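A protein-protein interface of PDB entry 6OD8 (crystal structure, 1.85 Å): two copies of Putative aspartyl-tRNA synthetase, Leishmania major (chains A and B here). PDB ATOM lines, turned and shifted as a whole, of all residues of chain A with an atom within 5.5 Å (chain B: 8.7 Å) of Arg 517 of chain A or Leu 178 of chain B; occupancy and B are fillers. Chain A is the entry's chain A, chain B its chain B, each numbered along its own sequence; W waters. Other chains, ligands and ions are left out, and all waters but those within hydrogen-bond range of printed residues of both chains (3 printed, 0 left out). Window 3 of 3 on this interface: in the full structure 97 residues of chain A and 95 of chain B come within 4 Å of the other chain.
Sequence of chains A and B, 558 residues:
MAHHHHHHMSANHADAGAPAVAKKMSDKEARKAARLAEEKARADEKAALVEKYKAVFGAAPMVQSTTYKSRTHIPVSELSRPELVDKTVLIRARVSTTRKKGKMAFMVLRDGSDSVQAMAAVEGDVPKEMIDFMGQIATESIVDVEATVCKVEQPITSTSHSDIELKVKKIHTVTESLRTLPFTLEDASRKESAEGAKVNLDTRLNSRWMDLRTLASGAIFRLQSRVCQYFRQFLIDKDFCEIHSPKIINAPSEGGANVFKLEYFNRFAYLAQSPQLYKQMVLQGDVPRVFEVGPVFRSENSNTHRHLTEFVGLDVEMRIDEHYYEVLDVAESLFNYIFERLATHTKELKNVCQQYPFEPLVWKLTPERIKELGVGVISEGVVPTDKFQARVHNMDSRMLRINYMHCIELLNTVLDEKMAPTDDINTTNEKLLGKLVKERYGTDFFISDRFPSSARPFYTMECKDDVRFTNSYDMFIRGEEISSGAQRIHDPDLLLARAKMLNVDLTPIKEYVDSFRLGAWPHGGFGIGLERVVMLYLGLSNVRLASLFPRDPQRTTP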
ATOM      1  N   PRO A 492       4.864 -30.468 -15.828  1.00  0.00           N
ATOM      2  CA  PRO A 492       5.598 -31.679 -15.405  1.00  0.00           C
ATOM      3  C   PRO A 492       5.484 -31.990 -13.920  1.00  0.00           C
ATOM      4  O   PRO A 492       5.398 -33.169 -13.538  1.00  0.00           O
ATOM      5  CB  PRO A 492       7.047 -31.358 -15.797  1.00  0.00           C
ATOM      6  CG  PRO A 492       6.944 -30.266 -16.809  1.00  0.00           C
ATOM      7  CD  PRO A 492       5.751 -29.461 -16.431  1.00  0.00           C
ATOM      8  N   ASP A 493       5.502 -30.967 -13.063  1.00  0.00           N
ATOM      9  CA  ASP A 493       5.526 -31.235 -11.629  1.00  0.00           C
ATOM     10  C   ASP A 493       4.179 -31.737 -11.140  1.00  0.00           C
ATOM     11  O   ASP A 493       4.120 -32.682 -10.338  1.00  0.00           O
ATOM     12  CB  ASP A 493       5.967 -29.982 -10.873  1.00  0.00           C
ATOM     13  CG  ASP A 493       7.397 -29.593 -11.202  1.00  0.00           C
ATOM     14  OD1 ASP A 493       8.322 -30.177 -10.602  1.00  0.00           O
ATOM     15  OD2 ASP A 493       7.596 -28.744 -12.101  1.00  0.00           O
ATOM     16  N   LEU A 496       3.808 -35.394 -12.199  1.00  0.00           N
ATOM     17  CA  LEU A 496       4.453 -36.330 -11.276  1.00  0.00           C
ATOM     18  C   LEU A 496       3.675 -36.436  -9.965  1.00  0.00           C
ATOM     19  O   LEU A 496       3.541 -37.529  -9.398  1.00  0.00           O
ATOM     20  CB  LEU A 496       5.902 -35.904 -11.023  1.00  0.00           C
ATOM     21  CG  LEU A 496       6.893 -36.062 -12.185  1.00  0.00           C
ATOM     22  CD1 LEU A 496       8.183 -35.315 -11.896  1.00  0.00           C
ATOM     23  CD2 LEU A 496       7.182 -37.537 -12.465  1.00  0.00           C
ATOM     24  N   VAL A 513       7.362 -37.412 -19.730  1.00  0.00           N
ATOM     25  CA  VAL A 513       7.409 -36.318 -18.753  1.00  0.00           C
ATOM     26  C   VAL A 513       8.345 -35.212 -19.246  1.00  0.00           C
ATOM     27  O   VAL A 513       8.003 -34.023 -19.222  1.00  0.00           O
ATOM     28  CB  VAL A 513       7.851 -36.848 -17.376  1.00  0.00           C
ATOM     29  CG1 VAL A 513       7.976 -35.700 -16.383  1.00  0.00           C
ATOM     30  CG2 VAL A 513       6.876 -37.920 -16.848  1.00  0.00           C
ATOM     31  N   ASP A 514       9.529 -35.598 -19.730  1.00  0.00           N
ATOM     32  CA  ASP A 514      10.503 -34.630 -20.232  1.00  0.00           C
ATOM     33  C   ASP A 514       9.950 -33.795 -21.384  1.00  0.00           C
ATOM     34  O   ASP A 514      10.401 -32.657 -21.591  1.00  0.00           O
ATOM     35  CB  ASP A 514      11.767 -35.353 -20.701  1.00  0.00           C
ATOM     36  CG  ASP A 514      12.656 -35.776 -19.556  1.00  0.00           C
ATOM     37  OD1 ASP A 514      12.358 -35.411 -18.389  1.00  0.00           O
ATOM     38  OD2 ASP A 514      13.652 -36.484 -19.832  1.00  0.00           O
ATOM     39  N   SER A 515       9.012 -34.340 -22.161  1.00  0.00           N
ATOM     40  CA  SER A 515       8.474 -33.586 -23.295  1.00  0.00           C
ATOM     41  C   SER A 515       7.674 -32.363 -22.873  1.00  0.00           C
ATOM     42  O   SER A 515       7.382 -31.517 -23.725  1.00  0.00           O
ATOM     43  CB  SER A 515       7.601 -34.472 -24.196  1.00  0.00           C
ATOM     44  OG  SER A 515       6.309 -34.720 -23.646  1.00  0.00           O
ATOM     45  N   PHE A 516       7.320 -32.244 -21.592  1.00  0.00           N
ATOM     46  CA  PHE A 516       6.576 -31.085 -21.114  1.00  0.00           C
ATOM     47  C   PHE A 516       7.461 -30.044 -20.455  1.00  0.00           C
ATOM     48  O   PHE A 516       6.937 -29.057 -19.921  1.00  0.00           O
ATOM     49  CB  PHE A 516       5.490 -31.526 -20.124  1.00  0.00           C
ATOM     50  CG  PHE A 516       4.571 -32.572 -20.672  1.00  0.00           C
ATOM     51  CD1 PHE A 516       3.679 -32.267 -21.704  1.00  0.00           C
ATOM     52  CD2 PHE A 516       4.611 -33.870 -20.185  1.00  0.00           C
ATOM     53  CE1 PHE A 516       2.828 -33.245 -22.224  1.00  0.00           C
ATOM     54  CE2 PHE A 516       3.737 -34.858 -20.684  1.00  0.00           C
ATOM     55  CZ  PHE A 516       2.858 -34.534 -21.719  1.00  0.00           C
ATOM     56  N   ARG A 517       8.781 -30.264 -20.424  1.00  0.00           N
ATOM     57  CA  ARG A 517       9.657 -29.425 -19.617  1.00  0.00           C
ATOM     58  C   ARG A 517      10.210 -28.231 -20.380  1.00  0.00           C
ATOM     59  O   ARG A 517      10.707 -27.298 -19.752  1.00  0.00           O
ATOM     60  CB  ARG A 517      10.817 -30.251 -19.065  1.00  0.00           C
ATOM     61  CG  ARG A 517      10.403 -31.289 -17.998  1.00  0.00           C
ATOM     62  CD  ARG A 517      11.674 -31.945 -17.457  1.00  0.00           C
ATOM     63  NE  ARG A 517      11.440 -33.173 -16.707  1.00  0.00           N
ATOM     64  CZ  ARG A 517      11.006 -33.212 -15.451  1.00  0.00           C
ATOM     65  NH1 ARG A 517      10.840 -34.386 -14.852  1.00  0.00           N
ATOM     66  NH2 ARG A 517      10.703 -32.089 -14.799  1.00  0.00           N
ATOM     67  N   LEU A 518      10.113 -28.227 -21.710  1.00  0.00           N
ATOM     68  CA  LEU A 518      10.685 -27.179 -22.560  1.00  0.00           C
ATOM     69  C   LEU A 518       9.588 -26.279 -23.124  1.00  0.00           C
ATOM     70  O   LEU A 518       9.606 -25.895 -24.300  1.00  0.00           O
ATOM     71  CB  LEU A 518      11.506 -27.791 -23.699  1.00  0.00           C
ATOM     72  CG  LEU A 518      12.583 -28.801 -23.278  1.00  0.00           C
ATOM     73  CD1 LEU A 518      13.300 -29.374 -24.498  1.00  0.00           C
ATOM     74  CD2 LEU A 518      13.584 -28.178 -22.299  1.00  0.00           C
ATOM     75  N   GLY A 519       8.627 -25.938 -22.276  1.00  0.00           N
ATOM     76  CA  GLY A 519       7.434 -25.223 -22.667  1.00  0.00           C
ATOM     77  C   GLY A 519       6.400 -26.191 -23.198  1.00  0.00           C
ATOM     78  O   GLY A 519       6.700 -26.982 -24.105  1.00  0.00           O
ATOM     79  N   ARG B  94       5.284 -19.472 -28.822  1.00  0.00           N
ATOM     80  CA  ARG B  94       6.560 -19.786 -28.198  1.00  0.00           C
ATOM     81  C   ARG B  94       7.492 -18.600 -28.274  1.00  0.00           C
ATOM     82  O   ARG B  94       7.506 -17.871 -29.265  1.00  0.00           O
ATOM     83  CB  ARG B  94       7.245 -20.956 -28.886  1.00  0.00           C
ATOM     84  CG  ARG B  94       6.564 -22.234 -28.671  1.00  0.00           C
ATOM     85  CD  ARG B  94       7.568 -23.295 -28.381  1.00  0.00           C
ATOM     86  NE  ARG B  94       6.913 -24.588 -28.289  1.00  0.00           N
ATOM     87  CZ  ARG B  94       6.898 -25.319 -27.190  1.00  0.00           C
ATOM     88  NH1 ARG B  94       7.532 -24.895 -26.104  1.00  0.00           N
ATOM     89  NH2 ARG B  94       6.298 -26.489 -27.205  1.00  0.00           N
ATOM     90  N   ILE B 137      12.312 -13.969 -19.850  1.00  0.00           N
ATOM     91  CA  ILE B 137      11.545 -15.184 -20.089  1.00  0.00           C
ATOM     92  C   ILE B 137      12.421 -16.202 -20.807  1.00  0.00           C
ATOM     93  O   ILE B 137      13.152 -15.868 -21.752  1.00  0.00           O
ATOM     94  CB  ILE B 137      10.286 -14.871 -20.914  1.00  0.00           C
ATOM     95  CG1 ILE B 137       9.342 -13.965 -20.126  1.00  0.00           C
ATOM     96  CG2 ILE B 137       9.577 -16.162 -21.308  1.00  0.00           C
ATOM     97  CD1 ILE B 137       8.196 -13.459 -20.965  1.00  0.00           C
ATOM     98  N   ALA B 138      12.353 -17.453 -20.365  1.00  0.00           N
ATOM     99  CA  ALA B 138      13.216 -18.481 -20.930  1.00  0.00           C
ATOM    100  C   ALA B 138      12.802 -18.799 -22.363  1.00  0.00           C
ATOM    101  O   ALA B 138      11.615 -18.884 -22.682  1.00  0.00           O
ATOM    102  CB  ALA B 138      13.182 -19.759 -20.081  1.00  0.00           C
ATOM    103  N   THR B 139      13.802 -18.948 -23.230  1.00  0.00           N
ATOM    104  CA  THR B 139      13.580 -19.432 -24.593  1.00  0.00           C
ATOM    105  C   THR B 139      12.783 -20.721 -24.570  1.00  0.00           C
ATOM    106  O   THR B 139      13.092 -21.627 -23.795  1.00  0.00           O
ATOM    107  CB  THR B 139      14.934 -19.672 -25.277  1.00  0.00           C
ATOM    108  OG1 THR B 139      15.714 -18.480 -25.195  1.00  0.00           O
ATOM    109  CG2 THR B 139      14.755 -20.061 -26.732  1.00  0.00           C
ATOM    110  N   GLU B 140      11.778 -20.809 -25.450  1.00  0.00           N
ATOM    111  CA  GLU B 140      10.832 -21.916 -25.682  1.00  0.00           C
ATOM    112  C   GLU B 140       9.645 -21.869 -24.715  1.00  0.00           C
ATOM    113  O   GLU B 140       8.746 -22.713 -24.834  1.00  0.00           O
ATOM    114  CB  GLU B 140      11.465 -23.321 -25.618  1.00  0.00           C
ATOM    115  CG  GLU B 140      12.478 -23.621 -26.732  1.00  0.00           C
ATOM    116  CD  GLU B 140      11.904 -23.363 -28.120  1.00  0.00           C
ATOM    117  OE1 GLU B 140      10.936 -24.059 -28.520  1.00  0.00           O
ATOM    118  OE2 GLU B 140      12.399 -22.434 -28.795  1.00  0.00           O
ATOM    119  N   SER B 141       9.589 -20.907 -23.797  1.00  0.00           N
ATOM    120  CA  SER B 141       8.395 -20.736 -22.980  1.00  0.00           C
ATOM    121  C   SER B 141       7.197 -20.402 -23.863  1.00  0.00           C
ATOM    122  O   SER B 141       7.332 -19.825 -24.931  1.00  0.00           O
ATOM    123  CB  SER B 141       8.610 -19.626 -21.942  1.00  0.00           C
ATOM    124  OG  SER B 141       9.661 -19.961 -21.039  1.00  0.00           O
ATOM    125  N   THR B 175       3.377 -21.558 -19.876  1.00  0.00           N
ATOM    126  CA  THR B 175       4.304 -22.474 -19.228  1.00  0.00           C
ATOM    127  C   THR B 175       5.724 -21.979 -19.461  1.00  0.00           C
ATOM    128  O   THR B 175       6.023 -21.384 -20.502  1.00  0.00           O
ATOM    129  CB  THR B 175       4.147 -23.909 -19.742  1.00  0.00           C
ATOM    130  OG1 THR B 175       4.309 -23.934 -21.165  1.00  0.00           O
ATOM    131  CG2 THR B 175       2.763 -24.465 -19.387  1.00  0.00           C
ATOM    132  N   GLU B 176       6.591 -22.200 -18.473  1.00  0.00           N
ATOM    133  CA  GLU B 176       7.985 -21.773 -18.540  1.00  0.00           C
ATOM    134  C   GLU B 176       8.846 -22.945 -18.974  1.00  0.00           C
ATOM    135  O   GLU B 176       8.694 -24.054 -18.449  1.00  0.00           O
ATOM    136  CB  GLU B 176       8.472 -21.251 -17.184  1.00  0.00           C
ATOM    137  CG  GLU B 176       7.744 -20.009 -16.732  1.00  0.00           C
ATOM    138  CD  GLU B 176       8.037 -19.645 -15.276  1.00  0.00           C
ATOM    139  OE1 GLU B 176       8.487 -20.527 -14.510  1.00  0.00           O
ATOM    140  OE2 GLU B 176       7.806 -18.480 -14.908  1.00  0.00           O
ATOM    141  N   SER B 177       9.735 -22.704 -19.934  1.00  0.00           N
ATOM    142  CA  SER B 177      10.697 -23.722 -20.332  1.00  0.00           C
ATOM    143  C   SER B 177      11.858 -23.767 -19.343  1.00  0.00           C
ATOM    144  O   SER B 177      12.200 -22.760 -18.731  1.00  0.00           O
ATOM    145  CB  SER B 177      11.231 -23.434 -21.739  1.00  0.00           C
ATOM    146  OG  SER B 177      12.210 -24.382 -22.095  1.00  0.00           O
ATOM    147  N   LEU B 178      12.453 -24.950 -19.175  1.00  0.00           N
ATOM    148  CA  LEU B 178      13.774 -25.019 -18.553  1.00  0.00           C
ATOM    149  C   LEU B 178      14.712 -24.076 -19.280  1.00  0.00           C
ATOM    150  O   LEU B 178      14.601 -23.885 -20.491  1.00  0.00           O
ATOM    151  CB  LEU B 178      14.354 -26.434 -18.614  1.00  0.00           C
ATOM    152  CG  LEU B 178      13.645 -27.532 -17.829  1.00  0.00           C
ATOM    153  CD1 LEU B 178      14.324 -28.872 -18.083  1.00  0.00           C
ATOM    154  CD2 LEU B 178      13.633 -27.200 -16.363  1.00  0.00           C
ATOM    155  N   ARG B 179      15.653 -23.487 -18.540  1.00  0.00           N
ATOM    156  CA  ARG B 179      16.602 -22.576 -19.177  1.00  0.00           C
ATOM    157  C   ARG B 179      17.765 -23.304 -19.849  1.00  0.00           C
ATOM    158  O   ARG B 179      18.458 -22.704 -20.677  1.00  0.00           O
ATOM    159  CB  ARG B 179      17.101 -21.547 -18.162  1.00  0.00           C
ATOM    160  CG  ARG B 179      15.986 -20.592 -17.749  1.00  0.00           C
ATOM    161  CD  ARG B 179      16.455 -19.521 -16.785  1.00  0.00           C
ATOM    162  NE  ARG B 179      15.343 -18.676 -16.348  1.00  0.00           N
ATOM    163  CZ  ARG B 179      14.905 -17.616 -17.020  1.00  0.00           C
ATOM    164  NH1 ARG B 179      15.488 -17.271 -18.161  1.00  0.00           N
ATOM    165  NH2 ARG B 179      13.884 -16.907 -16.560  1.00  0.00           N
ATOM    166  N   THR B 180      17.971 -24.580 -19.534  1.00  0.00           N
ATOM    167  CA  THR B 180      18.926 -25.436 -20.227  1.00  0.00           C
ATOM    168  C   THR B 180      18.175 -26.236 -21.287  1.00  0.00           C
ATOM    169  O   THR B 180      17.361 -27.099 -20.955  1.00  0.00           O
ATOM    170  CB  THR B 180      19.621 -26.377 -19.247  1.00  0.00           C
ATOM    171  OG1 THR B 180      20.278 -25.619 -18.224  1.00  0.00           O
ATOM    172  CG2 THR B 180      20.643 -27.239 -19.969  1.00  0.00           C
ATOM    173  N   LEU B 181      18.461 -25.972 -22.531  1.00  0.00           N
ATOM    174  CA  LEU B 181      17.882 -26.757 -23.613  1.00  0.00           C
ATOM    175  C   LEU B 181      18.828 -27.893 -24.002  1.00  0.00           C
ATOM    176  O   LEU B 181      20.045 -27.759 -23.863  1.00  0.00           O
ATOM    177  CB  LEU B 181      17.628 -25.864 -24.821  1.00  0.00           C
ATOM    178  CG  LEU B 181      16.729 -24.639 -24.635  1.00  0.00           C
ATOM    179  CD1 LEU B 181      16.662 -23.844 -25.932  1.00  0.00           C
ATOM    180  CD2 LEU B 181      15.341 -25.087 -24.224  1.00  0.00           C
ATOM    181  N   PRO B 182      18.306 -29.026 -24.485  1.00  0.00           N
ATOM    182  CA  PRO B 182      19.198 -30.093 -24.993  1.00  0.00           C
ATOM    183  C   PRO B 182      20.030 -29.679 -26.203  1.00  0.00           C
ATOM    184  O   PRO B 182      21.070 -30.293 -26.453  1.00  0.00           O
ATOM    185  CB  PRO B 182      18.222 -31.218 -25.363  1.00  0.00           C
ATOM    186  CG  PRO B 182      16.958 -30.487 -25.717  1.00  0.00           C
ATOM    187  CD  PRO B 182      16.891 -29.352 -24.712  1.00  0.00           C
ATOM    188  N   TRP B 209      10.750 -33.957 -29.395  1.00  0.00           N
ATOM    189  CA  TRP B 209       9.757 -32.893 -29.257  1.00  0.00           C
ATOM    190  C   TRP B 209      10.373 -31.524 -29.525  1.00  0.00           C
ATOM    191  O   TRP B 209       9.684 -30.614 -29.998  1.00  0.00           O
ATOM    192  CB  TRP B 209       9.114 -32.935 -27.861  1.00  0.00           C
ATOM    193  CG  TRP B 209      10.107 -33.092 -26.750  1.00  0.00           C
ATOM    194  CD1 TRP B 209      10.676 -32.110 -26.003  1.00  0.00           C
ATOM    195  CD2 TRP B 209      10.622 -34.321 -26.256  1.00  0.00           C
ATOM    196  NE1 TRP B 209      11.536 -32.654 -25.080  1.00  0.00           N
ATOM    197  CE2 TRP B 209      11.524 -34.016 -25.222  1.00  0.00           C
ATOM    198  CE3 TRP B 209      10.419 -35.660 -26.605  1.00  0.00           C
ATOM    199  CZ2 TRP B 209      12.227 -34.998 -24.526  1.00  0.00           C
ATOM    200  CZ3 TRP B 209      11.108 -36.628 -25.916  1.00  0.00           C
ATOM    201  CH2 TRP B 209      11.999 -36.298 -24.886  1.00  0.00           C
ATOM    202  N   MET B 210      11.674 -31.366 -29.250  1.00  0.00           N
ATOM    203  CA  MET B 210      12.355 -30.119 -29.555  1.00  0.00           C
ATOM    204  C   MET B 210      12.699 -30.027 -31.038  1.00  0.00           C
ATOM    205  O   MET B 210      12.501 -28.983 -31.670  1.00  0.00           O
ATOM    206  CB  MET B 210      13.611 -30.003 -28.679  1.00  0.00           C
ATOM    207  CG  MET B 210      14.424 -28.763 -28.916  1.00  0.00           C
ATOM    208  SD  MET B 210      13.642 -27.305 -28.196  1.00  0.00           S
ATOM    209  CE  MET B 210      14.877 -26.086 -28.680  1.00  0.00           C
ATOM    210  N   ARG B 213      10.169 -28.863 -33.710  1.00  0.00           N
ATOM    211  CA  ARG B 213       9.872 -27.445 -33.811  1.00  0.00           C
ATOM    212  C   ARG B 213      10.643 -26.752 -34.923  1.00  0.00           C
ATOM    213  O   ARG B 213      10.295 -25.619 -35.260  1.00  0.00           O
ATOM    214  CB  ARG B 213      10.170 -26.757 -32.473  1.00  0.00           C
ATOM    215  CG  ARG B 213       9.477 -27.447 -31.324  1.00  0.00           C
ATOM    216  CD  ARG B 213       9.871 -26.826 -29.975  1.00  0.00           C
ATOM    217  NE  ARG B 213       9.379 -27.686 -28.909  1.00  0.00           N
ATOM    218  CZ  ARG B 213       9.628 -27.514 -27.619  1.00  0.00           C
ATOM    219  NH1 ARG B 213      10.364 -26.482 -27.213  1.00  0.00           N
ATOM    220  NH2 ARG B 213       9.116 -28.378 -26.739  1.00  0.00           N
HETATM  221  O   HOH W   1       7.298 -26.475 -19.676  1.00  0.00           O
HETATM  222  O   HOH W   2      12.881 -32.002 -22.609  1.00  0.00           O
HETATM  223  O   HOH W   3       8.484 -29.041 -23.974  1.00  0.00           O
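The backbone carbonyl oxygen of Leu 518 of chain A lies close to the backbone carbonyl oxygen of Glu 140 of chain B (3.3 Å). The backbone carbonyl oxygen (O) of Leu 518 of chain A sits at hydrogen-bond distance from the guanidinium group (NH1) of Arg 213 of chain B (3.1 Å). The guanidinium group of Arg 94 of chain B sits at hydrogen-bond distance from the backbone carbonyl oxygen of Gly 519 of chain A. The backbone carbonyl oxygen of Leu 518 of chain A sits at hydrogen-bond distance from the guanidinium group of Arg 94 of chain B, 2.9 Å away. N of Leu 178 of chain B is in hydrogen-bond range of O of Arg 517 of chain A (3.0 Å).
OD1 of Asp 514 of chain A lies within salt-bridge range of NE of Arg 517 of chain A (2.9 Å). NH1 of Arg 94 of chain B is in hydrogen-bond range of O of Glu 140 of chain B. The side-chain carboxylate of Glu 140 of chain B lies within salt-bridge range of the guanidinium group of Arg 213 of chain B, at 2.8 Å. SD of Met 210 of chain B sits at hydrogen-bond distance from NH1 of Arg 213 of chain B, at 3.5 Å. The backbone carbonyl oxygen (O) of Trp 209 of chain B is in hydrogen-bond range of the guanidinium group (NE) of Arg 213 of chain B. The side-chain hydroxyl (OG) of Ser 177 of chain B sits close to the backbone carbonyl oxygen (O) of Thr 139 of chain B (3.4 Å).
Among the printed residues, pairs that only touch across the chains: Leu 518 of chain A with Ser 177 of chain B, Gly 519 of chain A with Glu 140 of chain B, Leu 518 of chain A with Pro 182 of chain B, Gly 519 of chain A with Ser 177 of chain B, Arg 517 of chain A with Ser 177 of chain B, Ser 515 of chain A with Trp 209 of chain B, Asp 514 of chain A with Trp 209 of chain B, Gly 519 of chain A with Thr 175 of chain B, Leu 518 of chain A with Trp 209 of chain B and Gly 519 of chain A with Arg 213 of chain B.
Printed residues of chain B within 4 Å of Asp 514 of chain A: Trp 209. Arg 517 of chain A touches just these residues of chain B: Ser 177 and Leu 178. Printed residues of chain A within 4 Å of Glu 140 of chain B: Leu 518 and Gly 519. Leu 178 of chain B touches one residue of chain A. Of the printed residues of chain A, Trp 209 of chain B touches Asp 514, Ser 515 and Leu 518. The nearest printed residue of chain A that does not touch Arg 94 of chain B is Ser 515 of chain A (6.2 Å).
Of the 10 printed residues of chain A, 5 touch a printed residue of chain B. Along chain A the printed residues that touch a printed residue of chain B span positions 514 to 519. Of the 17 printed residues of chain B, 8 touch a printed residue of chain A. Printed residues of chain B that touch a printed residue of chain A: Arg 94, Glu 140, Thr 175, Ser 177, Leu 178, Pro 182, Trp 209 and Arg 213. Hydrophobic or aromatic side chains of chain B within 4 Å of the printed part of chain A: Leu 178, Pro 182 and Trp 209. Among the printed residues, 15 pairs touch across the chains.
No position is printed for both chains. Of the 15 pairs that touch across the chains among the printed residues, none has its exchanged pair printed and touching as well.
Water W1 lies within hydrogen-bond range of O of Phe 516 of chain A (2.6 Å), N of Gly 519 of chain A (3.0 Å) and O of Glu 176 of chain B (3.1 Å). Water W3 lies within hydrogen-bond range of O of Ser 515 of chain A, O of Gly 519 of chain A, N of Leu 518 of chain A and NH2 of Arg 213 of chain B. Water W2 lies within hydrogen-bond range of O of Asp 514 of chain A (2.8 Å) and NE1 of Trp 209 of chain B (2.9 Å).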
